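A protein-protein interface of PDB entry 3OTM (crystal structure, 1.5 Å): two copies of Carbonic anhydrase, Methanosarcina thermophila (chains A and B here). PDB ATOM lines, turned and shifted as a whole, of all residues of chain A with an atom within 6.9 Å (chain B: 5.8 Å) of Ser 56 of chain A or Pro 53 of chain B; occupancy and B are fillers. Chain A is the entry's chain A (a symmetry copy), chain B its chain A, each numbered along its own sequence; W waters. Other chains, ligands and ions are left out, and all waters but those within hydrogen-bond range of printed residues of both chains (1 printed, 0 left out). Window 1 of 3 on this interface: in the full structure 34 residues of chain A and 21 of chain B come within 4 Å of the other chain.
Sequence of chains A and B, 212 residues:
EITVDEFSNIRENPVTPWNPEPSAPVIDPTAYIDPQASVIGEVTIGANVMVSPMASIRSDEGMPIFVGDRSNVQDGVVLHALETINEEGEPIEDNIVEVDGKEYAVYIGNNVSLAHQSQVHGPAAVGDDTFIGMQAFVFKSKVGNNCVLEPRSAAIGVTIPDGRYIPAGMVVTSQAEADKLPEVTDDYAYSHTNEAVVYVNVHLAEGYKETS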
ATOM      1  N   ARG A  11     -30.115 -12.928   0.071  1.00  0.00           N
ATOM      2  CA  ARG A  11     -30.372 -14.057  -0.818  1.00  0.00           C
ATOM      3  C   ARG A  11     -29.222 -15.052  -0.879  1.00  0.00           C
ATOM      4  O   ARG A  11     -28.071 -14.715  -0.621  1.00  0.00           O
ATOM      5  CB  ARG A  11     -30.600 -13.538  -2.241  1.00  0.00           C
ATOM      6  CG  ARG A  11     -31.668 -12.479  -2.347  1.00  0.00           C
ATOM      7  CD  ARG A  11     -31.485 -11.664  -3.603  1.00  0.00           C
ATOM      8  NE  ARG A  11     -31.332 -12.507  -4.783  1.00  0.00           N
ATOM      9  CZ  ARG A  11     -31.046 -12.039  -5.992  1.00  0.00           C
ATOM     10  NH1 ARG A  11     -30.886 -10.742  -6.167  1.00  0.00           N
ATOM     11  NH2 ARG A  11     -30.921 -12.863  -7.021  1.00  0.00           N
ATOM     12  N   GLN A  36     -32.745  -1.482   1.092  1.00  0.00           N
ATOM     13  CA  GLN A  36     -32.302  -1.155  -0.243  1.00  0.00           C
ATOM     14  C   GLN A  36     -30.830  -1.485  -0.476  1.00  0.00           C
ATOM     15  O   GLN A  36     -30.261  -1.071  -1.478  1.00  0.00           O
ATOM     16  CB  GLN A  36     -32.618   0.316  -0.581  1.00  0.00           C
ATOM     17  CG  GLN A  36     -34.136   0.532  -0.728  1.00  0.00           C
ATOM     18  CD  GLN A  36     -34.548   1.969  -1.031  1.00  0.00           C
ATOM     19  OE1 GLN A  36     -34.706   2.769  -0.133  1.00  0.00           O
ATOM     20  NE2 GLN A  36     -34.757   2.267  -2.288  1.00  0.00           N
ATOM     21  N   ALA A  37     -30.244  -2.287   0.402  1.00  0.00           N
ATOM     22  CA  ALA A  37     -28.958  -2.935   0.145  1.00  0.00           C
ATOM     23  C   ALA A  37     -29.218  -4.316  -0.396  1.00  0.00           C
ATOM     24  O   ALA A  37     -30.338  -4.834  -0.305  1.00  0.00           O
ATOM     25  CB  ALA A  37     -28.138  -3.018   1.408  1.00  0.00           C
ATOM     26  N   SER A  38     -28.201  -4.933  -0.976  1.00  0.00           N
ATOM     27  CA  SER A  38     -28.268  -6.304  -1.478  1.00  0.00           C
ATOM     28  C   SER A  38     -27.126  -7.097  -0.856  1.00  0.00           C
ATOM     29  O   SER A  38     -25.975  -6.662  -0.922  1.00  0.00           O
ATOM     30  CB  SER A  38     -28.132  -6.299  -2.990  1.00  0.00           C
ATOM     31  OG  SER A  38     -28.145  -7.618  -3.494  1.00  0.00           O
ATOM     32  N   VAL A  39     -27.419  -8.267  -0.281  1.00  0.00           N
ATOM     33  CA  VAL A  39     -26.418  -9.140   0.287  1.00  0.00           C
ATOM     34  C   VAL A  39     -26.708 -10.542  -0.231  1.00  0.00           C
ATOM     35  O   VAL A  39     -27.763 -11.124   0.057  1.00  0.00           O
ATOM     36  CB  VAL A  39     -26.459  -9.167   1.824  1.00  0.00           C
ATOM     37  CG1 VAL A  39     -25.327  -9.986   2.380  1.00  0.00           C
ATOM     38  CG2 VAL A  39     -26.359  -7.748   2.369  1.00  0.00           C
ATOM     39  N   ILE A  40     -25.787 -11.078  -1.004  1.00  0.00           N
ATOM     40  CA  ILE A  40     -25.980 -12.356  -1.689  1.00  0.00           C
ATOM     41  C   ILE A  40     -24.859 -13.328  -1.383  1.00  0.00           C
ATOM     42  O   ILE A  40     -23.700 -13.001  -1.534  1.00  0.00           O
ATOM     43  CB  ILE A  40     -25.999 -12.141  -3.213  1.00  0.00           C
ATOM     44  CG1 ILE A  40     -27.208 -11.311  -3.636  1.00  0.00           C
ATOM     45  CG2 ILE A  40     -26.031 -13.488  -3.954  1.00  0.00           C
ATOM     46  CD1 ILE A  40     -27.173 -10.892  -5.107  1.00  0.00           C
ATOM     47  N   VAL A  51     -25.078  -1.659   7.188  1.00  0.00           N
ATOM     48  CA  VAL A  51     -25.018  -1.739   5.742  1.00  0.00           C
ATOM     49  C   VAL A  51     -26.078  -0.787   5.188  1.00  0.00           C
ATOM     50  O   VAL A  51     -27.278  -0.929   5.444  1.00  0.00           O
ATOM     51  CB  VAL A  51     -25.225  -3.161   5.229  1.00  0.00           C
ATOM     52  CG1 VAL A  51     -25.134  -3.209   3.710  1.00  0.00           C
ATOM     53  CG2 VAL A  51     -24.169  -4.106   5.783  1.00  0.00           C
ATOM     54  N   SER A  52     -25.620   0.224   4.449  1.00  0.00           N
ATOM     55  CA  SER A  52     -26.434   1.348   4.002  1.00  0.00           C
ATOM     56  C   SER A  52     -27.136   1.093   2.673  1.00  0.00           C
ATOM     57  O   SER A  52     -26.840   0.129   1.965  1.00  0.00           O
ATOM     58  CB  SER A  52     -25.525   2.553   3.803  1.00  0.00           C
ATOM     59  OG  SER A  52     -25.038   3.009   5.034  1.00  0.00           O
ATOM     60  N   PRO A  53     -28.071   1.969   2.302  1.00  0.00           N
ATOM     61  CA  PRO A  53     -28.772   1.850   1.013  1.00  0.00           C
ATOM     62  C   PRO A  53     -27.809   1.766  -0.152  1.00  0.00           C
ATOM     63  O   PRO A  53     -26.781   2.443  -0.196  1.00  0.00           O
ATOM     64  CB  PRO A  53     -29.606   3.141   0.949  1.00  0.00           C
ATOM     65  CG  PRO A  53     -29.810   3.553   2.375  1.00  0.00           C
ATOM     66  CD  PRO A  53     -28.585   3.097   3.111  1.00  0.00           C
ATOM     67  N   MET A  54     -28.161   0.911  -1.114  1.00  0.00           N
ATOM     68  CA  MET A  54     -27.471   0.788  -2.392  1.00  0.00           C
ATOM     69  C   MET A  54     -26.136   0.086  -2.321  1.00  0.00           C
ATOM     70  O   MET A  54     -25.456  -0.043  -3.359  1.00  0.00           O
ATOM     71  CB  MET A  54     -27.329   2.125  -3.115  1.00  0.00           C
ATOM     72  CG  MET A  54     -28.548   2.987  -3.155  1.00  0.00           C
ATOM     73  SD  MET A  54     -30.025   2.171  -3.832  1.00  0.00           S
ATOM     74  CE  MET A  54     -31.264   3.367  -3.328  1.00  0.00           C
ATOM     75  N   ALA A  55     -25.754  -0.424  -1.151  1.00  0.00           N
ATOM     76  CA  ALA A  55     -24.573  -1.273  -1.090  1.00  0.00           C
ATOM     77  C   ALA A  55     -24.888  -2.617  -1.700  1.00  0.00           C
ATOM     78  O   ALA A  55     -26.012  -3.105  -1.609  1.00  0.00           O
ATOM     79  CB  ALA A  55     -24.110  -1.430   0.340  1.00  0.00           C
ATOM     80  N   SER A  56     -23.890  -3.218  -2.325  1.00  0.00           N
ATOM     81  CA  SER A  56     -24.022  -4.540  -2.900  1.00  0.00           C
ATOM     82  C   SER A  56     -22.876  -5.387  -2.426  1.00  0.00           C
ATOM     83  O   SER A  56     -21.717  -5.125  -2.779  1.00  0.00           O
ATOM     84  CB  SER A  56     -24.043  -4.479  -4.419  1.00  0.00           C
ATOM     85  OG  SER A  56     -24.265  -5.814  -4.896  1.00  0.00           O
ATOM     86  N   ILE A  57     -23.179  -6.406  -1.626  1.00  0.00           N
ATOM     87  CA  ILE A  57     -22.205  -7.361  -1.146  1.00  0.00           C
ATOM     88  C   ILE A  57     -22.558  -8.692  -1.802  1.00  0.00           C
ATOM     89  O   ILE A  57     -23.608  -9.245  -1.533  1.00  0.00           O
ATOM     90  CB  ILE A  57     -22.241  -7.504   0.378  1.00  0.00           C
ATOM     91  CG1 ILE A  57     -22.045  -6.137   1.029  1.00  0.00           C
ATOM     92  CG2 ILE A  57     -21.199  -8.496   0.813  1.00  0.00           C
ATOM     93  CD1 ILE A  57     -22.200  -6.168   2.589  1.00  0.00           C
ATOM     94  N   ARG A  58     -21.727  -9.170  -2.704  1.00  0.00           N
ATOM     95  CA  ARG A  58     -22.110 -10.263  -3.580  1.00  0.00           C
ATOM     96  C   ARG A  58     -21.010 -11.303  -3.580  1.00  0.00           C
ATOM     97  O   ARG A  58     -19.919 -11.072  -4.081  1.00  0.00           O
ATOM     98  CB  ARG A  58     -22.417  -9.746  -4.995  1.00  0.00           C
ATOM     99  CG  ARG A  58     -22.923 -10.818  -5.964  1.00  0.00           C
ATOM    100  CD  ARG A  58     -23.676 -10.217  -7.151  1.00  0.00           C
ATOM    101  NE  ARG A  58     -22.825  -9.389  -8.010  1.00  0.00           N
ATOM    102  CZ  ARG A  58     -22.173  -9.805  -9.084  1.00  0.00           C
ATOM    103  NH1 ARG A  58     -22.184 -11.083  -9.450  1.00  0.00           N
ATOM    104  NH2 ARG A  58     -21.475  -8.939  -9.805  1.00  0.00           N
ATOM    105  N   VAL A  73     -20.532  -0.468   6.042  1.00  0.00           N
ATOM    106  CA  VAL A  73     -20.538  -0.584   4.579  1.00  0.00           C
ATOM    107  C   VAL A  73     -21.509   0.457   4.069  1.00  0.00           C
ATOM    108  O   VAL A  73     -22.716   0.275   4.167  1.00  0.00           O
ATOM    109  CB  VAL A  73     -20.972  -1.981   4.166  1.00  0.00           C
ATOM    110  CG1 VAL A  73     -20.923  -2.125   2.655  1.00  0.00           C
ATOM    111  CG2 VAL A  73     -20.073  -3.049   4.810  1.00  0.00           C
ATOM    112  N   GLN A  74     -20.983   1.582   3.594  1.00  0.00           N
ATOM    113  CA  GLN A  74     -21.797   2.760   3.337  1.00  0.00           C
ATOM    114  C   GLN A  74     -22.437   2.732   1.941  1.00  0.00           C
ATOM    115  O   GLN A  74     -22.338   1.756   1.197  1.00  0.00           O
ATOM    116  CB  GLN A  74     -20.968   4.024   3.576  1.00  0.00           C
ATOM    117  CG  GLN A  74     -20.566   4.154   5.056  1.00  0.00           C
ATOM    118  CD  GLN A  74     -19.709   5.353   5.296  1.00  0.00           C
ATOM    119  OE1 GLN A  74     -19.713   6.318   4.541  1.00  0.00           O
ATOM    120  NE2 GLN A  74     -18.937   5.296   6.369  1.00  0.00           N
ATOM    121  N   GLY A  76     -23.779   2.684  -1.641  1.00  0.00           N
ATOM    122  CA  GLY A  76     -23.189   2.440  -2.942  1.00  0.00           C
ATOM    123  C   GLY A  76     -21.877   1.673  -2.928  1.00  0.00           C
ATOM    124  O   GLY A  76     -21.236   1.583  -3.984  1.00  0.00           O
ATOM    125  N   VAL A  77     -21.441   1.133  -1.791  1.00  0.00           N
ATOM    126  CA  VAL A  77     -20.221   0.361  -1.752  1.00  0.00           C
ATOM    127  C   VAL A  77     -20.444  -0.995  -2.396  1.00  0.00           C
ATOM    128  O   VAL A  77     -21.521  -1.578  -2.273  1.00  0.00           O
ATOM    129  CB  VAL A  77     -19.775   0.195  -0.295  1.00  0.00           C
ATOM    130  CG1 VAL A  77     -18.683  -0.881  -0.135  1.00  0.00           C
ATOM    131  CG2 VAL A  77     -19.257   1.527   0.210  1.00  0.00           C
ATOM    132  N   VAL A  78     -19.464  -1.487  -3.124  1.00  0.00           N
ATOM    133  CA  VAL A  78     -19.522  -2.818  -3.713  1.00  0.00           C
ATOM    134  C   VAL A  78     -18.408  -3.685  -3.155  1.00  0.00           C
ATOM    135  O   VAL A  78     -17.246  -3.254  -3.099  1.00  0.00           O
ATOM    136  CB  VAL A  78     -19.401  -2.753  -5.255  1.00  0.00           C
ATOM    137  CG1 VAL A  78     -19.370  -4.163  -5.892  1.00  0.00           C
ATOM    138  CG2 VAL A  78     -20.593  -1.979  -5.841  1.00  0.00           C
ATOM    139  N   LEU A  79     -18.771  -4.897  -2.726  1.00  0.00           N
ATOM    140  CA  LEU A  79     -17.828  -5.957  -2.388  1.00  0.00           C
ATOM    141  C   LEU A  79     -18.128  -7.143  -3.300  1.00  0.00           C
ATOM    142  O   LEU A  79     -19.257  -7.591  -3.391  1.00  0.00           O
ATOM    143  CB  LEU A  79     -17.956  -6.397  -0.926  1.00  0.00           C
ATOM    144  CG  LEU A  79     -17.805  -5.309   0.141  1.00  0.00           C
ATOM    145  CD1 LEU A  79     -17.998  -5.911   1.535  1.00  0.00           C
ATOM    146  CD2 LEU A  79     -16.460  -4.677   0.036  1.00  0.00           C
ATOM    147  N   HIS A  80     -17.117  -7.614  -4.002  1.00  0.00           N
ATOM    148  CA  HIS A  80     -17.234  -8.769  -4.903  1.00  0.00           C
ATOM    149  C   HIS A  80     -15.829  -9.355  -5.034  1.00  0.00           C
ATOM    150  O   HIS A  80     -14.876  -8.745  -4.553  1.00  0.00           O
ATOM    151  CB  HIS A  80     -17.779  -8.346  -6.283  1.00  0.00           C
ATOM    152  CG  HIS A  80     -18.163  -9.502  -7.152  1.00  0.00           C
ATOM    153  ND1 HIS A  80     -17.541  -9.779  -8.353  1.00  0.00           N
ATOM    154  CD2 HIS A  80     -19.128 -10.439  -6.997  1.00  0.00           C
ATOM    155  CE1 HIS A  80     -18.085 -10.873  -8.876  1.00  0.00           C
ATOM    156  NE2 HIS A  80     -19.053 -11.283  -8.079  1.00  0.00           N
ATOM    157  N   ASP B  34     -31.361  -8.511 -12.430  1.00  0.00           N
ATOM    158  CA  ASP B  34     -31.560  -8.587 -11.000  1.00  0.00           C
ATOM    159  C   ASP B  34     -32.742  -7.734 -10.576  1.00  0.00           C
ATOM    160  O   ASP B  34     -32.951  -6.651 -11.119  1.00  0.00           O
ATOM    161  CB  ASP B  34     -30.300  -8.127 -10.270  1.00  0.00           C
ATOM    162  CG  ASP B  34     -30.340  -8.470  -8.809  1.00  0.00           C
ATOM    163  OD1 ASP B  34     -29.943  -9.623  -8.508  1.00  0.00           O
ATOM    164  OD2 ASP B  34     -30.759  -7.624  -7.992  1.00  0.00           O
ATOM    165  N   GLN B  36     -32.990  -5.840  -8.152  1.00  0.00           N
ATOM    166  CA  GLN B  36     -32.522  -4.579  -7.625  1.00  0.00           C
ATOM    167  C   GLN B  36     -31.717  -3.775  -8.642  1.00  0.00           C
ATOM    168  O   GLN B  36     -31.079  -2.795  -8.280  1.00  0.00           O
ATOM    169  CB  GLN B  36     -31.737  -4.791  -6.314  1.00  0.00           C
ATOM    170  CG  GLN B  36     -32.676  -5.239  -5.178  1.00  0.00           C
ATOM    171  CD  GLN B  36     -31.982  -5.504  -3.846  1.00  0.00           C
ATOM    172  OE1 GLN B  36     -31.484  -6.586  -3.614  1.00  0.00           O
ATOM    173  NE2 GLN B  36     -31.994  -4.529  -2.973  1.00  0.00           N
ATOM    174  N   ALA B  37     -31.811  -4.141  -9.913  1.00  0.00           N
ATOM    175  CA  ALA B  37     -31.362  -3.291 -11.015  1.00  0.00           C
ATOM    176  C   ALA B  37     -32.544  -2.513 -11.530  1.00  0.00           C
ATOM    177  O   ALA B  37     -33.699  -2.835 -11.226  1.00  0.00           O
ATOM    178  CB  ALA B  37     -30.764  -4.122 -12.123  1.00  0.00           C
ATOM    179  N   MET B  50     -25.983 -10.670 -18.043  1.00  0.00           N
ATOM    180  CA  MET B  50     -26.218 -10.574 -16.621  1.00  0.00           C
ATOM    181  C   MET B  50     -26.218  -9.109 -16.214  1.00  0.00           C
ATOM    182  O   MET B  50     -25.244  -8.407 -16.471  1.00  0.00           O
ATOM    183  CB  MET B  50     -25.096 -11.319 -15.906  1.00  0.00           C
ATOM    184  CG  MET B  50     -25.035 -11.066 -14.431  1.00  0.00           C
ATOM    185  SD  MET B  50     -26.102 -12.183 -13.592  1.00  0.00           S
ATOM    186  CE  MET B  50     -25.840 -11.579 -11.926  1.00  0.00           C
ATOM    187  N   VAL B  51     -27.306  -8.639 -15.623  1.00  0.00           N
ATOM    188  CA  VAL B  51     -27.401  -7.297 -15.082  1.00  0.00           C
ATOM    189  C   VAL B  51     -27.522  -7.426 -13.563  1.00  0.00           C
ATOM    190  O   VAL B  51     -28.461  -8.028 -13.034  1.00  0.00           O
ATOM    191  CB  VAL B  51     -28.572  -6.515 -15.668  1.00  0.00           C
ATOM    192  CG1 VAL B  51     -28.627  -5.106 -15.094  1.00  0.00           C
ATOM    193  CG2 VAL B  51     -28.449  -6.389 -17.180  1.00  0.00           C
ATOM    194  N   SER B  52     -26.531  -6.885 -12.855  1.00  0.00           N
ATOM    195  CA  SER B  52     -26.349  -7.072 -11.420  1.00  0.00           C
ATOM    196  C   SER B  52     -27.103  -6.049 -10.578  1.00  0.00           C
ATOM    197  O   SER B  52     -27.607  -5.046 -11.086  1.00  0.00           O
ATOM    198  CB  SER B  52     -24.871  -6.915 -11.096  1.00  0.00           C
ATOM    199  OG  SER B  52     -24.134  -7.980 -11.631  1.00  0.00           O
ATOM    200  N   PRO B  53     -27.178  -6.278  -9.267  1.00  0.00           N
ATOM    201  CA  PRO B  53     -27.834  -5.327  -8.353  1.00  0.00           C
ATOM    202  C   PRO B  53     -27.273  -3.928  -8.489  1.00  0.00           C
ATOM    203  O   PRO B  53     -26.069  -3.724  -8.654  1.00  0.00           O
ATOM    204  CB  PRO B  53     -27.529  -5.912  -6.964  1.00  0.00           C
ATOM    205  CG  PRO B  53     -27.305  -7.377  -7.189  1.00  0.00           C
ATOM    206  CD  PRO B  53     -26.710  -7.492  -8.561  1.00  0.00           C
ATOM    207  N   MET B  54     -28.176  -2.950  -8.418  1.00  0.00           N
ATOM    208  CA  MET B  54     -27.843  -1.532  -8.364  1.00  0.00           C
ATOM    209  C   MET B  54     -27.379  -0.943  -9.676  1.00  0.00           C
ATOM    210  O   MET B  54     -27.043   0.257  -9.725  1.00  0.00           O
ATOM    211  CB  MET B  54     -26.848  -1.202  -7.255  1.00  0.00           C
ATOM    212  CG  MET B  54     -27.115  -1.822  -5.922  1.00  0.00           C
ATOM    213  SD  MET B  54     -28.777  -1.495  -5.261  1.00  0.00           S
ATOM    214  CE  MET B  54     -28.795  -2.703  -3.933  1.00  0.00           C
ATOM    215  N   ALA B  55     -27.397  -1.723 -10.756  1.00  0.00           N
ATOM    216  CA  ALA B  55     -27.146  -1.138 -12.066  1.00  0.00           C
ATOM    217  C   ALA B  55     -28.345  -0.327 -12.493  1.00  0.00           C
ATOM    218  O   ALA B  55     -29.481  -0.660 -12.166  1.00  0.00           O
ATOM    219  CB  ALA B  55     -26.844  -2.220 -13.077  1.00  0.00           C
ATOM    220  N   GLN B  74     -22.325  -4.904 -14.426  1.00  0.00           N
ATOM    221  CA  GLN B  74     -22.096  -5.277 -13.040  1.00  0.00           C
ATOM    222  C   GLN B  74     -22.651  -4.234 -12.056  1.00  0.00           C
ATOM    223  O   GLN B  74     -23.305  -3.262 -12.436  1.00  0.00           O
ATOM    224  CB  GLN B  74     -20.608  -5.556 -12.817  1.00  0.00           C
ATOM    225  CG  GLN B  74     -20.146  -6.784 -13.624  1.00  0.00           C
ATOM    226  CD  GLN B  74     -18.683  -7.036 -13.463  1.00  0.00           C
ATOM    227  OE1 GLN B  74     -18.054  -6.627 -12.495  1.00  0.00           O
ATOM    228  NE2 GLN B  74     -18.113  -7.720 -14.441  1.00  0.00           N
ATOM    229  N   ASP B  75     -22.413  -4.475 -10.786  1.00  0.00           N
ATOM    230  CA  ASP B  75     -23.120  -3.765  -9.715  1.00  0.00           C
ATOM    231  C   ASP B  75     -22.811  -2.292  -9.776  1.00  0.00           C
ATOM    232  O   ASP B  75     -21.655  -1.883  -9.882  1.00  0.00           O
ATOM    233  CB  ASP B  75     -22.713  -4.263  -8.304  1.00  0.00           C
ATOM    234  CG  ASP B  75     -22.595  -5.775  -8.199  1.00  0.00           C
ATOM    235  OD1 ASP B  75     -21.734  -6.318  -8.912  1.00  0.00           O
ATOM    236  OD2 ASP B  75     -23.308  -6.383  -7.383  1.00  0.00           O
ATOM    237  N   GLY B  76     -23.844  -1.465  -9.703  1.00  0.00           N
ATOM    238  CA  GLY B  76     -23.667  -0.026  -9.657  1.00  0.00           C
ATOM    239  C   GLY B  76     -23.269   0.622 -10.972  1.00  0.00           C
ATOM    240  O   GLY B  76     -22.935   1.814 -10.964  1.00  0.00           O
ATOM    241  N   VAL B  77     -23.271  -0.101 -12.092  1.00  0.00           N
ATOM    242  CA  VAL B  77     -22.939   0.495 -13.365  1.00  0.00           C
ATOM    243  C   VAL B  77     -24.084   1.372 -13.841  1.00  0.00           C
ATOM    244  O   VAL B  77     -25.252   1.054 -13.620  1.00  0.00           O
ATOM    245  CB  VAL B  77     -22.655  -0.614 -14.384  1.00  0.00           C
ATOM    246  CG1 VAL B  77     -22.621  -0.087 -15.831  1.00  0.00           C
ATOM    247  CG2 VAL B  77     -21.326  -1.258 -14.042  1.00  0.00           C
HETATM  248  O   HOH W   1     -32.112  -1.318  -3.578  1.00  0.00           O
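N of Met 54 of chain A sits at hydrogen-bond distance from O of Gln 36 of chain A.
NH1 of Arg 58 of chain A is in hydrogen-bond range of NE2 of His 80 of chain A (3.4 Å).
O of Ala 55 of chain A sits at hydrogen-bond distance from N of Ser 38 of chain A, 2.9 Å away.
N of Ile 57 of chain A is in hydrogen-bond range of O of Ser 38 of chain A (2.9 Å).
The backbone NH of Asp 34 of chain B lies within hydrogen-bond range of the backbone carbonyl oxygen of Val 51 of chain B (3.0 Å).
N of Ser 56 of chain A is in hydrogen-bond range of O of Val 77 of chain A (2.9 Å).
The guanidinium group (NH2) of Arg 58 of chain A is in salt-bridge range of the side-chain carboxylate (OD1) of Asp 75 of chain B.
OG of Ser 38 of chain A sits close to OE1 of Gln 36 of chain B, 3.5 Å away.
The side-chain amide nitrogen of Gln 36 of chain B sits at hydrogen-bond distance from the backbone carbonyl oxygen of Ala 37 of chain A, at 3.2 Å.
OG of Ser 52 of chain B is in hydrogen-bond range of NH2 of Arg 58 of chain A, 3.4 Å away.
The side-chain carboxylate of Asp 34 of chain B lies within salt-bridge range of the guanidinium group of Arg 11 of chain A.
The side-chain hydroxyl (OG) of Ser 56 of chain A is in hydrogen-bond range of the side-chain carboxylate (OD2) of Asp 75 of chain B (2.7 Å).
Of the 21 printed residues of chain A, 9 touch a printed residue of chain B.
Hydrophobic or aromatic side chains of chain A that line the printed part of chain B: Val 78.
Printed residues of chain B that touch a printed residue of chain A: Asp 34, Gln 36, Ser 52, Pro 53, Met 54 and Asp 75.
Among the printed residues, pairs that only touch across the chains: Gln 36 of chain A with Met 54 of chain B, Met 54 of chain A with Met 54 of chain B, Ala 55 of chain A with Met 54 of chain B, Ser 38 of chain A with Met 54 of chain B, Ser 38 of chain A with Pro 53 of chain B, Ser 56 of chain A with Pro 53 of chain B, Ala 37 of chain A with Met 54 of chain B and Val 78 of chain A with Asp 75 of chain B.
Water W1 lies within hydrogen-bond range of the backbone carbonyl oxygen of Gln 36 of chain A (2.8 Å), the side-chain amide nitrogen of Gln 36 of chain B (3.3 Å) and the side-chain sulfur of Met 54 of chain B (3.7 Å).
Gln 36 of chain A touches Met 54 of chain B, but with the chains exchanged Met 54 of chain A does not touch Gln 36 of chain B (6.7 Å).
Ala 37 of chain A touches Gln 36 of chain B, but with the chains exchanged Gln 36 of chain A does not touch Ala 37 of chain B (9.1 Å).
Ala 37 of chain A touches Met 54 of chain B, but with the chains exchanged Met 54 of chain A does not touch Ala 37 of chain B (8.9 Å).
Met 54 of chain A touches its own counterpart, Met 54 of chain B.
Positions printed for both chains: 36, 37, 51, 52, 53, 54, 55, 74, 76 and 77.
Of the 14 pairs that touch across the chains among the printed residues, 1 has its exchanged pair printed and touching as well.
Of the printed residues of chain B, Gln 36 of chain A touches Met 54.
Of the printed residues of chain B, Ser 38 of chain A touches Gln 36 (3.4 Å), Pro 53 (3.8 Å) and Met 54 (3.8 Å).
Ser 52 of chain A touches none of the printed residues of chain B.
Ser 56 of chain A touches two residues of chain B.
Ile 57 of chain A touches none of the printed residues of chain B.
Of the printed residues of chain B, Arg 58 of chain A touches Ser 52 (3.4 Å) and Asp 75 (2.8 Å).
Printed residues of chain A within 4 Å of Asp 34 of chain B: Arg 11 (2.8 Å).
Printed residues of chain A within 4 Å of Pro 53 of chain B: Ser 38 (3.8 Å) and Ser 56 (3.9 Å).
The nearest residue of chain B that does not touch Ser 56 of chain A is Met 54 of chain B (4.3 Å).
The nearest printed residue of chain B that does not touch Met 54 of chain A is Pro 53 of chain B (6.5 Å).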
